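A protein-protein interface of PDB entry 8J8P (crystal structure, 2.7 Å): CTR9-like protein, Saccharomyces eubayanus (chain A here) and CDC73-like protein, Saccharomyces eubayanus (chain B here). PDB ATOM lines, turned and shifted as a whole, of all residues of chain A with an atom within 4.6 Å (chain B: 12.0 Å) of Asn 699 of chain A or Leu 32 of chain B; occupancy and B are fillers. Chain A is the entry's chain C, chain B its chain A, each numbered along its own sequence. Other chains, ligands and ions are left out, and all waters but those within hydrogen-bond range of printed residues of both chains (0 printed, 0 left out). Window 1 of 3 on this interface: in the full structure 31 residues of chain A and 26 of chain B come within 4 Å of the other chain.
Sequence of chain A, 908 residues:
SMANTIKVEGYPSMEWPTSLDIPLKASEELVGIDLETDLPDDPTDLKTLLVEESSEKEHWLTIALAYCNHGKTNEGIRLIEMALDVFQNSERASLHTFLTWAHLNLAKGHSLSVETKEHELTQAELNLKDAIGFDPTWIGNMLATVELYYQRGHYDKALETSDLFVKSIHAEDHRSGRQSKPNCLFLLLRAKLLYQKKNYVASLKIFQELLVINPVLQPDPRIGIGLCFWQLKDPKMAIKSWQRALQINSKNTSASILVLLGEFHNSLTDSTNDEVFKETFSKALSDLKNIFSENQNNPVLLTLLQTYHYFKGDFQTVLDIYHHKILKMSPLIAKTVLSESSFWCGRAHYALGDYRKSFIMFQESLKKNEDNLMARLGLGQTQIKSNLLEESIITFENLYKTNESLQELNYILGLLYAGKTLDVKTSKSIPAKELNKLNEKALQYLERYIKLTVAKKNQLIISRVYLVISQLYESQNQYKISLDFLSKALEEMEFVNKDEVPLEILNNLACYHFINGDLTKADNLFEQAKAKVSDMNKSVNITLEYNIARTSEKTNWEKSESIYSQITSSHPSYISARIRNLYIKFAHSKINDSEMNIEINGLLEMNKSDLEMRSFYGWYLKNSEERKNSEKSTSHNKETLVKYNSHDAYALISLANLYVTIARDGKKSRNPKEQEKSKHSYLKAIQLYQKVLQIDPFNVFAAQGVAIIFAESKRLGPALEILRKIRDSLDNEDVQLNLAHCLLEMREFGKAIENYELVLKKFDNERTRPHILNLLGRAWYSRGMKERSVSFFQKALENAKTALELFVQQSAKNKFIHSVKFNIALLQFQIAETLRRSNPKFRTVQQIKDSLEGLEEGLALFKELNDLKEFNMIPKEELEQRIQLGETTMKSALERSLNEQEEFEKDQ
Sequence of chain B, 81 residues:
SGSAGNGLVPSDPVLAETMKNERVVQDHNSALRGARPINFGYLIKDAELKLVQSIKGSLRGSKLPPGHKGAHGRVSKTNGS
The backbone NH (N) of Tyr 650 of chain A sits close to the side-chain amide nitrogen (ND2) of Asn 29 of chain B, at 2.8 Å.
NH1 of Arg 33 of chain B lies within salt-bridge range of OD1 of Asp 696 of chain A, 3.2 Å away.
The backbone carbonyl oxygen of Leu 32 of chain B lies close to the side-chain amide oxygen of Asn 699 of chain A, at 3.0 Å.
The backbone NH of Val 700 of chain A sits at hydrogen-bond distance from the backbone carbonyl oxygen of Leu 32 of chain B (3.2 Å).
The side-chain carboxylate (OD1) of Asp 696 of chain A lies within hydrogen-bond range of the backbone NH (N) of Phe 698 of chain A, at 3.3 Å.
The backbone NH of Phe 701 of chain A lies within hydrogen-bond range of the side-chain amide oxygen of Asn 699 of chain A, 2.9 Å away.
A ring nitrogen (NE2) of His 28 of chain B sits at hydrogen-bond distance from the side-chain amide oxygen (OD1) of Asn 29 of chain B (2.5 Å).
The guanidinium group of Arg 33 of chain B lies within hydrogen-bond range of the backbone carbonyl oxygen of Ser 30 of chain B, 2.8 Å away.
N of Gly 41 of chain B sits close to ND2 of Asn 39 of chain B.
Tyr 650 of chain A touches Leu 32 of chain B.
Pro 697 of chain A touches Asn 39 of chain B (CB to OD1, 3.2 Å).
CB of Phe 40 of chain B touches O of Pro 697 of chain A, 3.6 Å away.
CB of Arg 33 of chain B touches O of Phe 698 of chain A (3.7 Å).
CB of Phe 698 of chain A touches CB of Pro 37 of chain B, at 3.9 Å.
Phe 698 of chain A touches Ile 38 of chain B.
Phe 698 of chain A touches Asn 39 of chain B (CD2 to CA, 3.6 Å).
Val 700 of chain A touches Arg 33 of chain B.
Ala 703 of chain A touches Phe 40 of chain B (CB to CD2, 3.97 Å).
Asn 699 of chain A touches just one residue of chain B: Leu 32.
Leu 32 of chain B touches just these residues of chain A: Tyr 650 (3.6 Å), Asn 699 (3.0 Å) and Val 700 (3.2 Å).
No residue of chain B comes within 4 Å of Val 692 of chain A.
Of chain B, only Arg 33 (3.2 Å) comes within 4 Å of Asp 696 of chain A.
Pro 697 of chain A touches just these residues of chain B: Asn 39 and Phe 40.
Phe 698 of chain A touches just these residues of chain B: Arg 33 (3.7 Å), Pro 37 (3.9 Å), Ile 38 (3.7 Å) and Asn 39 (3.6 Å).
Val 700 of chain A touches just these residues of chain B: Leu 32 (3.2 Å) and Arg 33 (3.6 Å).
Phe 701 of chain A touches none of the printed residues of chain B.
Ala 702 of chain A touches none of the printed residues of chain B.
Of the printed residues of chain A, Arg 33 of chain B touches Asp 696, Phe 698 and Val 700.
Of the printed residues of chain A, Asn 29 of chain B touches Tyr 650 (2.8 Å).
Of the printed residues of chain A, Ile 38 of chain B touches Phe 698.
Printed residues of chain A within 4 Å of Asn 39 of chain B: Pro 697 and Phe 698.
The nearest residue of chain A that does not touch Leu 32 of chain B is Phe 701 of chain A (4.1 Å).
Of the 20 printed residues of chain B, 7 touch a printed residue of chain A.
Hydrophobic or aromatic side chains of chain B that line the printed part of chain A: Leu 32, Pro 37 and Phe 40.
Of the 11 printed residues of chain A, 7 touch a printed residue of chain B.
Printed residues of chain A that touch a printed residue of chain B: Tyr 650, Asp 696, Pro 697, Phe 698, Asn 699, Val 700 and Ala 703.
Among the printed residues, 13 pairs touch across the chains.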
ATOM      1  N   TYR A 650       6.008  18.953 -14.587  1.00  0.00           N
ATOM      2  CA  TYR A 650       4.687  18.354 -14.386  1.00  0.00           C
ATOM      3  C   TYR A 650       4.039  17.880 -15.684  1.00  0.00           C
ATOM      4  O   TYR A 650       3.830  16.674 -15.889  1.00  0.00           O
ATOM      5  CB  TYR A 650       3.765  19.353 -13.676  1.00  0.00           C
ATOM      6  CG  TYR A 650       2.401  18.809 -13.286  1.00  0.00           C
ATOM      7  CD1 TYR A 650       1.370  18.717 -14.217  1.00  0.00           C
ATOM      8  CD2 TYR A 650       2.139  18.411 -11.982  1.00  0.00           C
ATOM      9  CE1 TYR A 650       0.125  18.227 -13.864  1.00  0.00           C
ATOM     10  CE2 TYR A 650       0.892  17.922 -11.619  1.00  0.00           C
ATOM     11  CZ  TYR A 650      -0.110  17.834 -12.564  1.00  0.00           C
ATOM     12  OH  TYR A 650      -1.350  17.350 -12.210  1.00  0.00           O
ATOM     13  N   ILE A 653       6.068  15.111 -17.462  1.00  0.00           N
ATOM     14  CA  ILE A 653       5.868  13.714 -17.090  1.00  0.00           C
ATOM     15  C   ILE A 653       4.454  13.243 -17.415  1.00  0.00           C
ATOM     16  O   ILE A 653       4.235  12.039 -17.597  1.00  0.00           O
ATOM     17  CB  ILE A 653       6.203  13.469 -15.603  1.00  0.00           C
ATOM     18  CG1 ILE A 653       5.172  14.126 -14.682  1.00  0.00           C
ATOM     19  CG2 ILE A 653       7.618  13.946 -15.283  1.00  0.00           C
ATOM     20  CD1 ILE A 653       4.207  13.151 -14.044  1.00  0.00           C
ATOM     21  N   VAL A 692      13.913  14.806 -16.698  1.00  0.00           N
ATOM     22  CA  VAL A 692      13.216  15.309 -15.510  1.00  0.00           C
ATOM     23  C   VAL A 692      13.839  14.780 -14.214  1.00  0.00           C
ATOM     24  O   VAL A 692      13.768  15.443 -13.174  1.00  0.00           O
ATOM     25  CB  VAL A 692      11.702  15.039 -15.586  1.00  0.00           C
ATOM     26  CG1 VAL A 692      11.080  14.924 -14.197  1.00  0.00           C
ATOM     27  CG2 VAL A 692      11.031  16.195 -16.333  1.00  0.00           C
ATOM     28  N   ASP A 696      15.285  17.499 -11.332  1.00  0.00           N
ATOM     29  CA  ASP A 696      14.948  17.322  -9.925  1.00  0.00           C
ATOM     30  C   ASP A 696      14.971  15.836  -9.590  1.00  0.00           C
ATOM     31  O   ASP A 696      14.040  15.102  -9.947  1.00  0.00           O
ATOM     32  CB  ASP A 696      13.579  17.929  -9.605  1.00  0.00           C
ATOM     33  CG  ASP A 696      13.141  17.671  -8.167  1.00  0.00           C
ATOM     34  OD1 ASP A 696      14.004  17.393  -7.306  1.00  0.00           O
ATOM     35  OD2 ASP A 696      11.924  17.752  -7.897  1.00  0.00           O
ATOM     36  N   PRO A 697      16.021  15.357  -8.916  1.00  0.00           N
ATOM     37  CA  PRO A 697      16.092  13.917  -8.614  1.00  0.00           C
ATOM     38  C   PRO A 697      14.954  13.418  -7.739  1.00  0.00           C
ATOM     39  O   PRO A 697      14.382  12.356  -8.023  1.00  0.00           O
ATOM     40  CB  PRO A 697      17.455  13.775  -7.916  1.00  0.00           C
ATOM     41  CG  PRO A 697      18.242  14.982  -8.336  1.00  0.00           C
ATOM     42  CD  PRO A 697      17.234  16.080  -8.495  1.00  0.00           C
ATOM     43  N   PHE A 698      14.599  14.167  -6.692  1.00  0.00           N
ATOM     44  CA  PHE A 698      13.669  13.683  -5.679  1.00  0.00           C
ATOM     45  C   PHE A 698      12.223  13.618  -6.151  1.00  0.00           C
ATOM     46  O   PHE A 698      11.361  13.227  -5.353  1.00  0.00           O
ATOM     47  CB  PHE A 698      13.736  14.556  -4.423  1.00  0.00           C
ATOM     48  CG  PHE A 698      15.126  14.992  -4.048  1.00  0.00           C
ATOM     49  CD1 PHE A 698      15.692  16.142  -4.585  1.00  0.00           C
ATOM     50  CD2 PHE A 698      15.875  14.236  -3.159  1.00  0.00           C
ATOM     51  CE1 PHE A 698      16.974  16.530  -4.229  1.00  0.00           C
ATOM     52  CE2 PHE A 698      17.153  14.619  -2.808  1.00  0.00           C
ATOM     53  CZ  PHE A 698      17.703  15.763  -3.339  1.00  0.00           C
ATOM     54  N   ASN A 699      11.931  13.993  -7.404  1.00  0.00           N
ATOM     55  CA  ASN A 699      10.577  13.846  -7.924  1.00  0.00           C
ATOM     56  C   ASN A 699      10.249  12.367  -7.901  1.00  0.00           C
ATOM     57  O   ASN A 699      10.824  11.569  -8.648  1.00  0.00           O
ATOM     58  CB  ASN A 699      10.428  14.441  -9.332  1.00  0.00           C
ATOM     59  CG  ASN A 699       9.120  14.017 -10.036  1.00  0.00           C
ATOM     60  OD1 ASN A 699       8.204  13.465  -9.424  1.00  0.00           O
ATOM     61  ND2 ASN A 699       9.019  14.343 -11.323  1.00  0.00           N
ATOM     62  N   VAL A 700       9.315  12.014  -7.029  1.00  0.00           N
ATOM     63  CA  VAL A 700       8.947  10.631  -6.811  1.00  0.00           C
ATOM     64  C   VAL A 700       8.375   9.978  -8.066  1.00  0.00           C
ATOM     65  O   VAL A 700       8.666   8.806  -8.341  1.00  0.00           O
ATOM     66  CB  VAL A 700       7.979  10.627  -5.619  1.00  0.00           C
ATOM     67  CG1 VAL A 700       7.058   9.473  -5.663  1.00  0.00           C
ATOM     68  CG2 VAL A 700       8.764  10.644  -4.294  1.00  0.00           C
ATOM     69  N   PHE A 701       7.621  10.727  -8.873  1.00  0.00           N
ATOM     70  CA  PHE A 701       6.800  10.096  -9.898  1.00  0.00           C
ATOM     71  C   PHE A 701       7.611   9.674 -11.121  1.00  0.00           C
ATOM     72  O   PHE A 701       7.277   8.669 -11.760  1.00  0.00           O
ATOM     73  CB  PHE A 701       5.651  11.028 -10.288  1.00  0.00           C
ATOM     74  CG  PHE A 701       4.601  11.185  -9.208  1.00  0.00           C
ATOM     75  CD1 PHE A 701       3.251  11.228  -9.516  1.00  0.00           C
ATOM     76  CD2 PHE A 701       4.974  11.285  -7.880  1.00  0.00           C
ATOM     77  CE1 PHE A 701       2.304  11.358  -8.510  1.00  0.00           C
ATOM     78  CE2 PHE A 701       4.039  11.422  -6.878  1.00  0.00           C
ATOM     79  CZ  PHE A 701       2.700  11.462  -7.191  1.00  0.00           C
ATOM     80  N   ALA A 702       8.677  10.403 -11.459  1.00  0.00           N
ATOM     81  CA  ALA A 702       9.655   9.864 -12.400  1.00  0.00           C
ATOM     82  C   ALA A 702      10.132   8.487 -11.950  1.00  0.00           C
ATOM     83  O   ALA A 702      10.267   7.567 -12.767  1.00  0.00           O
ATOM     84  CB  ALA A 702      10.832  10.828 -12.540  1.00  0.00           C
ATOM     85  N   ALA A 703      10.363   8.323 -10.642  1.00  0.00           N
ATOM     86  CA  ALA A 703      10.711   7.019 -10.089  1.00  0.00           C
ATOM     87  C   ALA A 703       9.643   5.972 -10.376  1.00  0.00           C
ATOM     88  O   ALA A 703       9.979   4.817 -10.661  1.00  0.00           O
ATOM     89  CB  ALA A 703      10.955   7.133  -8.582  1.00  0.00           C
ATOM     90  N   VAL B  25       4.544  28.650  -0.707  1.00  0.00           N
ATOM     91  CA  VAL B  25       5.167  27.704   0.213  1.00  0.00           C
ATOM     92  C   VAL B  25       5.816  26.559  -0.559  1.00  0.00           C
ATOM     93  O   VAL B  25       6.929  26.124  -0.230  1.00  0.00           O
ATOM     94  CB  VAL B  25       4.127  27.197   1.230  1.00  0.00           C
ATOM     95  CG1 VAL B  25       2.841  26.806   0.528  1.00  0.00           C
ATOM     96  CG2 VAL B  25       4.694  26.039   2.042  1.00  0.00           C
ATOM     97  N   GLN B  26       5.148  26.070  -1.609  1.00  0.00           N
ATOM     98  CA  GLN B  26       5.631  24.935  -2.387  1.00  0.00           C
ATOM     99  C   GLN B  26       5.020  25.028  -3.773  1.00  0.00           C
ATOM    100  O   GLN B  26       3.797  25.115  -3.900  1.00  0.00           O
ATOM    101  CB  GLN B  26       5.253  23.619  -1.707  1.00  0.00           C
ATOM    102  CG  GLN B  26       6.298  22.516  -1.809  1.00  0.00           C
ATOM    103  CD  GLN B  26       5.809  21.220  -1.184  1.00  0.00           C
ATOM    104  OE1 GLN B  26       6.596  20.321  -0.878  1.00  0.00           O
ATOM    105  NE2 GLN B  26       4.500  21.125  -0.980  1.00  0.00           N
ATOM    106  N   ASP B  27       5.862  24.998  -4.803  1.00  0.00           N
ATOM    107  CA  ASP B  27       5.376  25.119  -6.168  1.00  0.00           C
ATOM    108  C   ASP B  27       4.557  23.886  -6.558  1.00  0.00           C
ATOM    109  O   ASP B  27       4.425  22.921  -5.797  1.00  0.00           O
ATOM    110  CB  ASP B  27       6.542  25.308  -7.141  1.00  0.00           C
ATOM    111  CG  ASP B  27       7.596  26.267  -6.612  1.00  0.00           C
ATOM    112  OD1 ASP B  27       7.693  27.399  -7.134  1.00  0.00           O
ATOM    113  OD2 ASP B  27       8.324  25.886  -5.669  1.00  0.00           O
ATOM    114  N   HIS B  28       3.989  23.933  -7.764  1.00  0.00           N
ATOM    115  CA  HIS B  28       3.317  22.758  -8.310  1.00  0.00           C
ATOM    116  C   HIS B  28       4.314  21.738  -8.843  1.00  0.00           C
ATOM    117  O   HIS B  28       4.002  20.543  -8.905  1.00  0.00           O
ATOM    118  CB  HIS B  28       2.361  23.168  -9.425  1.00  0.00           C
ATOM    119  CG  HIS B  28       3.052  23.504 -10.708  1.00  0.00           C
ATOM    120  ND1 HIS B  28       2.629  23.028 -11.930  1.00  0.00           N
ATOM    121  CD2 HIS B  28       4.140  24.271 -10.958  1.00  0.00           C
ATOM    122  CE1 HIS B  28       3.426  23.487 -12.877  1.00  0.00           C
ATOM    123  NE2 HIS B  28       4.351  24.245 -12.315  1.00  0.00           N
ATOM    124  N   ASN B  29       5.499  22.191  -9.242  1.00  0.00           N
ATOM    125  CA  ASN B  29       6.572  21.326  -9.703  1.00  0.00           C
ATOM    126  C   ASN B  29       7.459  20.844  -8.568  1.00  0.00           C
ATOM    127  O   ASN B  29       8.383  20.060  -8.812  1.00  0.00           O
ATOM    128  CB  ASN B  29       7.427  22.059 -10.739  1.00  0.00           C
ATOM    129  CG  ASN B  29       6.862  21.950 -12.132  1.00  0.00           C
ATOM    130  OD1 ASN B  29       6.444  22.940 -12.731  1.00  0.00           O
ATOM    131  ND2 ASN B  29       6.831  20.735 -12.653  1.00  0.00           N
ATOM    132  N   SER B  30       7.206  21.295  -7.340  1.00  0.00           N
ATOM    133  CA  SER B  30       8.048  20.959  -6.207  1.00  0.00           C
ATOM    134  C   SER B  30       7.338  20.162  -5.120  1.00  0.00           C
ATOM    135  O   SER B  30       8.016  19.623  -4.238  1.00  0.00           O
ATOM    136  CB  SER B  30       8.648  22.236  -5.595  1.00  0.00           C
ATOM    137  OG  SER B  30       7.653  23.042  -4.992  1.00  0.00           O
ATOM    138  N   ALA B  31       6.011  20.064  -5.148  1.00  0.00           N
ATOM    139  CA  ALA B  31       5.302  19.186  -4.226  1.00  0.00           C
ATOM    140  C   ALA B  31       5.060  17.800  -4.811  1.00  0.00           C
ATOM    141  O   ALA B  31       4.360  16.989  -4.192  1.00  0.00           O
ATOM    142  CB  ALA B  31       3.973  19.811  -3.801  1.00  0.00           C
ATOM    143  N   LEU B  32       5.626  17.517  -5.984  1.00  0.00           N
ATOM    144  CA  LEU B  32       5.573  16.199  -6.600  1.00  0.00           C
ATOM    145  C   LEU B  32       6.636  15.285  -6.003  1.00  0.00           C
ATOM    146  O   LEU B  32       7.231  14.476  -6.720  1.00  0.00           O
ATOM    147  CB  LEU B  32       5.791  16.312  -8.112  1.00  0.00           C
ATOM    148  CG  LEU B  32       4.951  17.296  -8.923  1.00  0.00           C
ATOM    149  CD1 LEU B  32       5.619  17.581 -10.263  1.00  0.00           C
ATOM    150  CD2 LEU B  32       3.552  16.752  -9.131  1.00  0.00           C
ATOM    151  N   ARG B  33       6.906  15.412  -4.699  1.00  0.00           N
ATOM    152  CA  ARG B  33       8.076  14.768  -4.113  1.00  0.00           C
ATOM    153  C   ARG B  33       7.777  13.990  -2.835  1.00  0.00           C
ATOM    154  O   ARG B  33       8.716  13.514  -2.186  1.00  0.00           O
ATOM    155  CB  ARG B  33       9.168  15.810  -3.842  1.00  0.00           C
ATOM    156  CG  ARG B  33       9.485  16.685  -5.046  1.00  0.00           C
ATOM    157  CD  ARG B  33      10.810  17.408  -4.899  1.00  0.00           C
ATOM    158  NE  ARG B  33      10.631  18.804  -4.510  1.00  0.00           N
ATOM    159  CZ  ARG B  33      11.557  19.745  -4.662  1.00  0.00           C
ATOM    160  NH1 ARG B  33      12.728  19.439  -5.202  1.00  0.00           N
ATOM    161  NH2 ARG B  33      11.314  20.991  -4.278  1.00  0.00           N
ATOM    162  N   GLY B  34       6.513  13.834  -2.459  1.00  0.00           N
ATOM    163  CA  GLY B  34       6.193  13.049  -1.285  1.00  0.00           C
ATOM    164  C   GLY B  34       6.331  13.830   0.004  1.00  0.00           C
ATOM    165  O   GLY B  34       5.933  14.996   0.067  1.00  0.00           O
ATOM    166  N   ALA B  35       6.893  13.204   1.041  1.00  0.00           N
ATOM    167  CA  ALA B  35       7.018  13.854   2.345  1.00  0.00           C
ATOM    168  C   ALA B  35       8.359  13.645   3.028  1.00  0.00           C
ATOM    169  O   ALA B  35       8.749  14.498   3.832  1.00  0.00           O
ATOM    170  CB  ALA B  35       5.907  13.380   3.290  1.00  0.00           C
ATOM    171  N   ARG B  36       9.067  12.551   2.767  1.00  0.00           N
ATOM    172  CA  ARG B  36      10.443  12.369   3.220  1.00  0.00           C
ATOM    173  C   ARG B  36      11.270  11.954   1.992  1.00  0.00           C
ATOM    174  O   ARG B  36      11.612  10.790   1.827  1.00  0.00           O
ATOM    175  CB  ARG B  36      10.527  11.335   4.348  1.00  0.00           C
ATOM    176  CG  ARG B  36       9.652  10.100   4.158  1.00  0.00           C
ATOM    177  CD  ARG B  36       8.350  10.178   4.955  1.00  0.00           C
ATOM    178  NE  ARG B  36       7.538   8.972   4.785  1.00  0.00           N
ATOM    179  CZ  ARG B  36       6.328   8.789   5.311  1.00  0.00           C
ATOM    180  NH1 ARG B  36       5.761   9.735   6.049  1.00  0.00           N
ATOM    181  NH2 ARG B  36       5.678   7.653   5.092  1.00  0.00           N
ATOM    182  N   PRO B  37      11.594  12.925   1.138  1.00  0.00           N
ATOM    183  CA  PRO B  37      12.083  12.568  -0.211  1.00  0.00           C
ATOM    184  C   PRO B  37      13.370  11.762  -0.192  1.00  0.00           C
ATOM    185  O   PRO B  37      14.257  11.969   0.640  1.00  0.00           O
ATOM    186  CB  PRO B  37      12.295  13.943  -0.864  1.00  0.00           C
ATOM    187  CG  PRO B  37      12.420  14.906   0.272  1.00  0.00           C
ATOM    188  CD  PRO B  37      11.525  14.370   1.340  1.00  0.00           C
ATOM    189  N   ILE B  38      13.455  10.822  -1.131  1.00  0.00           N
ATOM    190  CA  ILE B  38      14.653  10.034  -1.390  1.00  0.00           C
ATOM    191  C   ILE B  38      15.240  10.497  -2.716  1.00  0.00           C
ATOM    192  O   ILE B  38      14.502  10.742  -3.677  1.00  0.00           O
ATOM    193  CB  ILE B  38      14.341   8.523  -1.431  1.00  0.00           C
ATOM    194  CG1 ILE B  38      13.786   8.041  -0.086  1.00  0.00           C
ATOM    195  CG2 ILE B  38      15.581   7.728  -1.829  1.00  0.00           C
ATOM    196  CD1 ILE B  38      14.839   7.527   0.879  1.00  0.00           C
ATOM    197  N   ASN B  39      16.563  10.634  -2.765  1.00  0.00           N
ATOM    198  CA  ASN B  39      17.219  10.974  -4.021  1.00  0.00           C
ATOM    199  C   ASN B  39      17.178   9.780  -4.964  1.00  0.00           C
ATOM    200  O   ASN B  39      17.543   8.661  -4.588  1.00  0.00           O
ATOM    201  CB  ASN B  39      18.667  11.403  -3.787  1.00  0.00           C
ATOM    202  CG  ASN B  39      19.503  11.340  -5.058  1.00  0.00           C
ATOM    203  OD1 ASN B  39      19.474  12.258  -5.880  1.00  0.00           O
ATOM    204  ND2 ASN B  39      20.245  10.249  -5.228  1.00  0.00           N
ATOM    205  N   PHE B  40      16.733  10.021  -6.195  1.00  0.00           N
ATOM    206  CA  PHE B  40      16.694   8.998  -7.231  1.00  0.00           C
ATOM    207  C   PHE B  40      17.703   9.286  -8.341  1.00  0.00           C
ATOM    208  O   PHE B  40      17.458   8.977  -9.511  1.00  0.00           O
ATOM    209  CB  PHE B  40      15.277   8.865  -7.789  1.00  0.00           C
ATOM    210  CG  PHE B  40      14.263   8.413  -6.765  1.00  0.00           C
ATOM    211  CD1 PHE B  40      14.250   7.101  -6.313  1.00  0.00           C
ATOM    212  CD2 PHE B  40      13.331   9.301  -6.249  1.00  0.00           C
ATOM    213  CE1 PHE B  40      13.324   6.683  -5.368  1.00  0.00           C
ATOM    214  CE2 PHE B  40      12.401   8.888  -5.305  1.00  0.00           C
ATOM    215  CZ  PHE B  40      12.400   7.577  -4.864  1.00  0.00           C
ATOM    216  N   GLY B  41      18.841   9.885  -7.983  1.00  0.00           N
ATOM    217  CA  GLY B  41      19.912  10.134  -8.931  1.00  0.00           C
ATOM    218  C   GLY B  41      20.671   8.894  -9.341  1.00  0.00           C
ATOM    219  O   GLY B  41      21.498   8.963 -10.257  1.00  0.00           O
ATOM    220  N   TYR B  42      20.419   7.766  -8.679  1.00  0.00           N
ATOM    221  CA  TYR B  42      21.003   6.507  -9.118  1.00  0.00           C
ATOM    222  C   TYR B  42      20.316   5.987 -10.375  1.00  0.00           C
ATOM    223  O   TYR B  42      20.940   5.282 -11.186  1.00  0.00           O
ATOM    224  CB  TYR B  42      20.951   5.501  -7.962  1.00  0.00           C
ATOM    225  CG  TYR B  42      19.566   5.185  -7.402  1.00  0.00           C
ATOM    226  CD1 TYR B  42      18.650   4.421  -8.140  1.00  0.00           C
ATOM    227  CD2 TYR B  42      19.169   5.658  -6.144  1.00  0.00           C
ATOM    228  CE1 TYR B  42      17.386   4.119  -7.632  1.00  0.00           C
ATOM    229  CE2 TYR B  42      17.928   5.368  -5.633  1.00  0.00           C
ATOM    230  CZ  TYR B  42      17.041   4.609  -6.350  1.00  0.00           C
ATOM    231  OH  TYR B  42      15.809   4.347  -5.806  1.00  0.00           O
ATOM    232  N   LEU B  43      19.055   6.375 -10.577  1.00  0.00           N
ATOM    233  CA  LEU B  43      18.275   5.875 -11.699  1.00  0.00           C
ATOM    234  C   LEU B  43      18.644   6.482 -13.053  1.00  0.00           C
ATOM    235  O   LEU B  43      18.325   5.866 -14.067  1.00  0.00           O
ATOM    236  CB  LEU B  43      16.786   6.060 -11.424  1.00  0.00           C
ATOM    237  CG  LEU B  43      16.119   4.902 -10.648  1.00  0.00           C
ATOM    238  CD1 LEU B  43      14.606   4.988 -10.765  1.00  0.00           C
ATOM    239  CD2 LEU B  43      16.581   3.610 -11.243  1.00  0.00           C
ATOM    240  N   ILE B  44      19.371   7.603 -13.121  1.00  0.00           N
ATOM    241  CA  ILE B  44      19.835   8.078 -14.433  1.00  0.00           C
ATOM    242  C   ILE B  44      20.790   7.071 -15.065  1.00  0.00           C
ATOM    243  O   ILE B  44      20.614   6.641 -16.217  1.00  0.00           O
ATOM    244  CB  ILE B  44      20.486   9.473 -14.329  1.00  0.00           C
ATOM    245  CG1 ILE B  44      21.028   9.922 -15.696  1.00  0.00           C
ATOM    246  CG2 ILE B  44      21.539   9.540 -13.235  1.00  0.00           C
ATOM    247  CD1 ILE B  44      19.980  10.577 -16.550  1.00  0.00           C
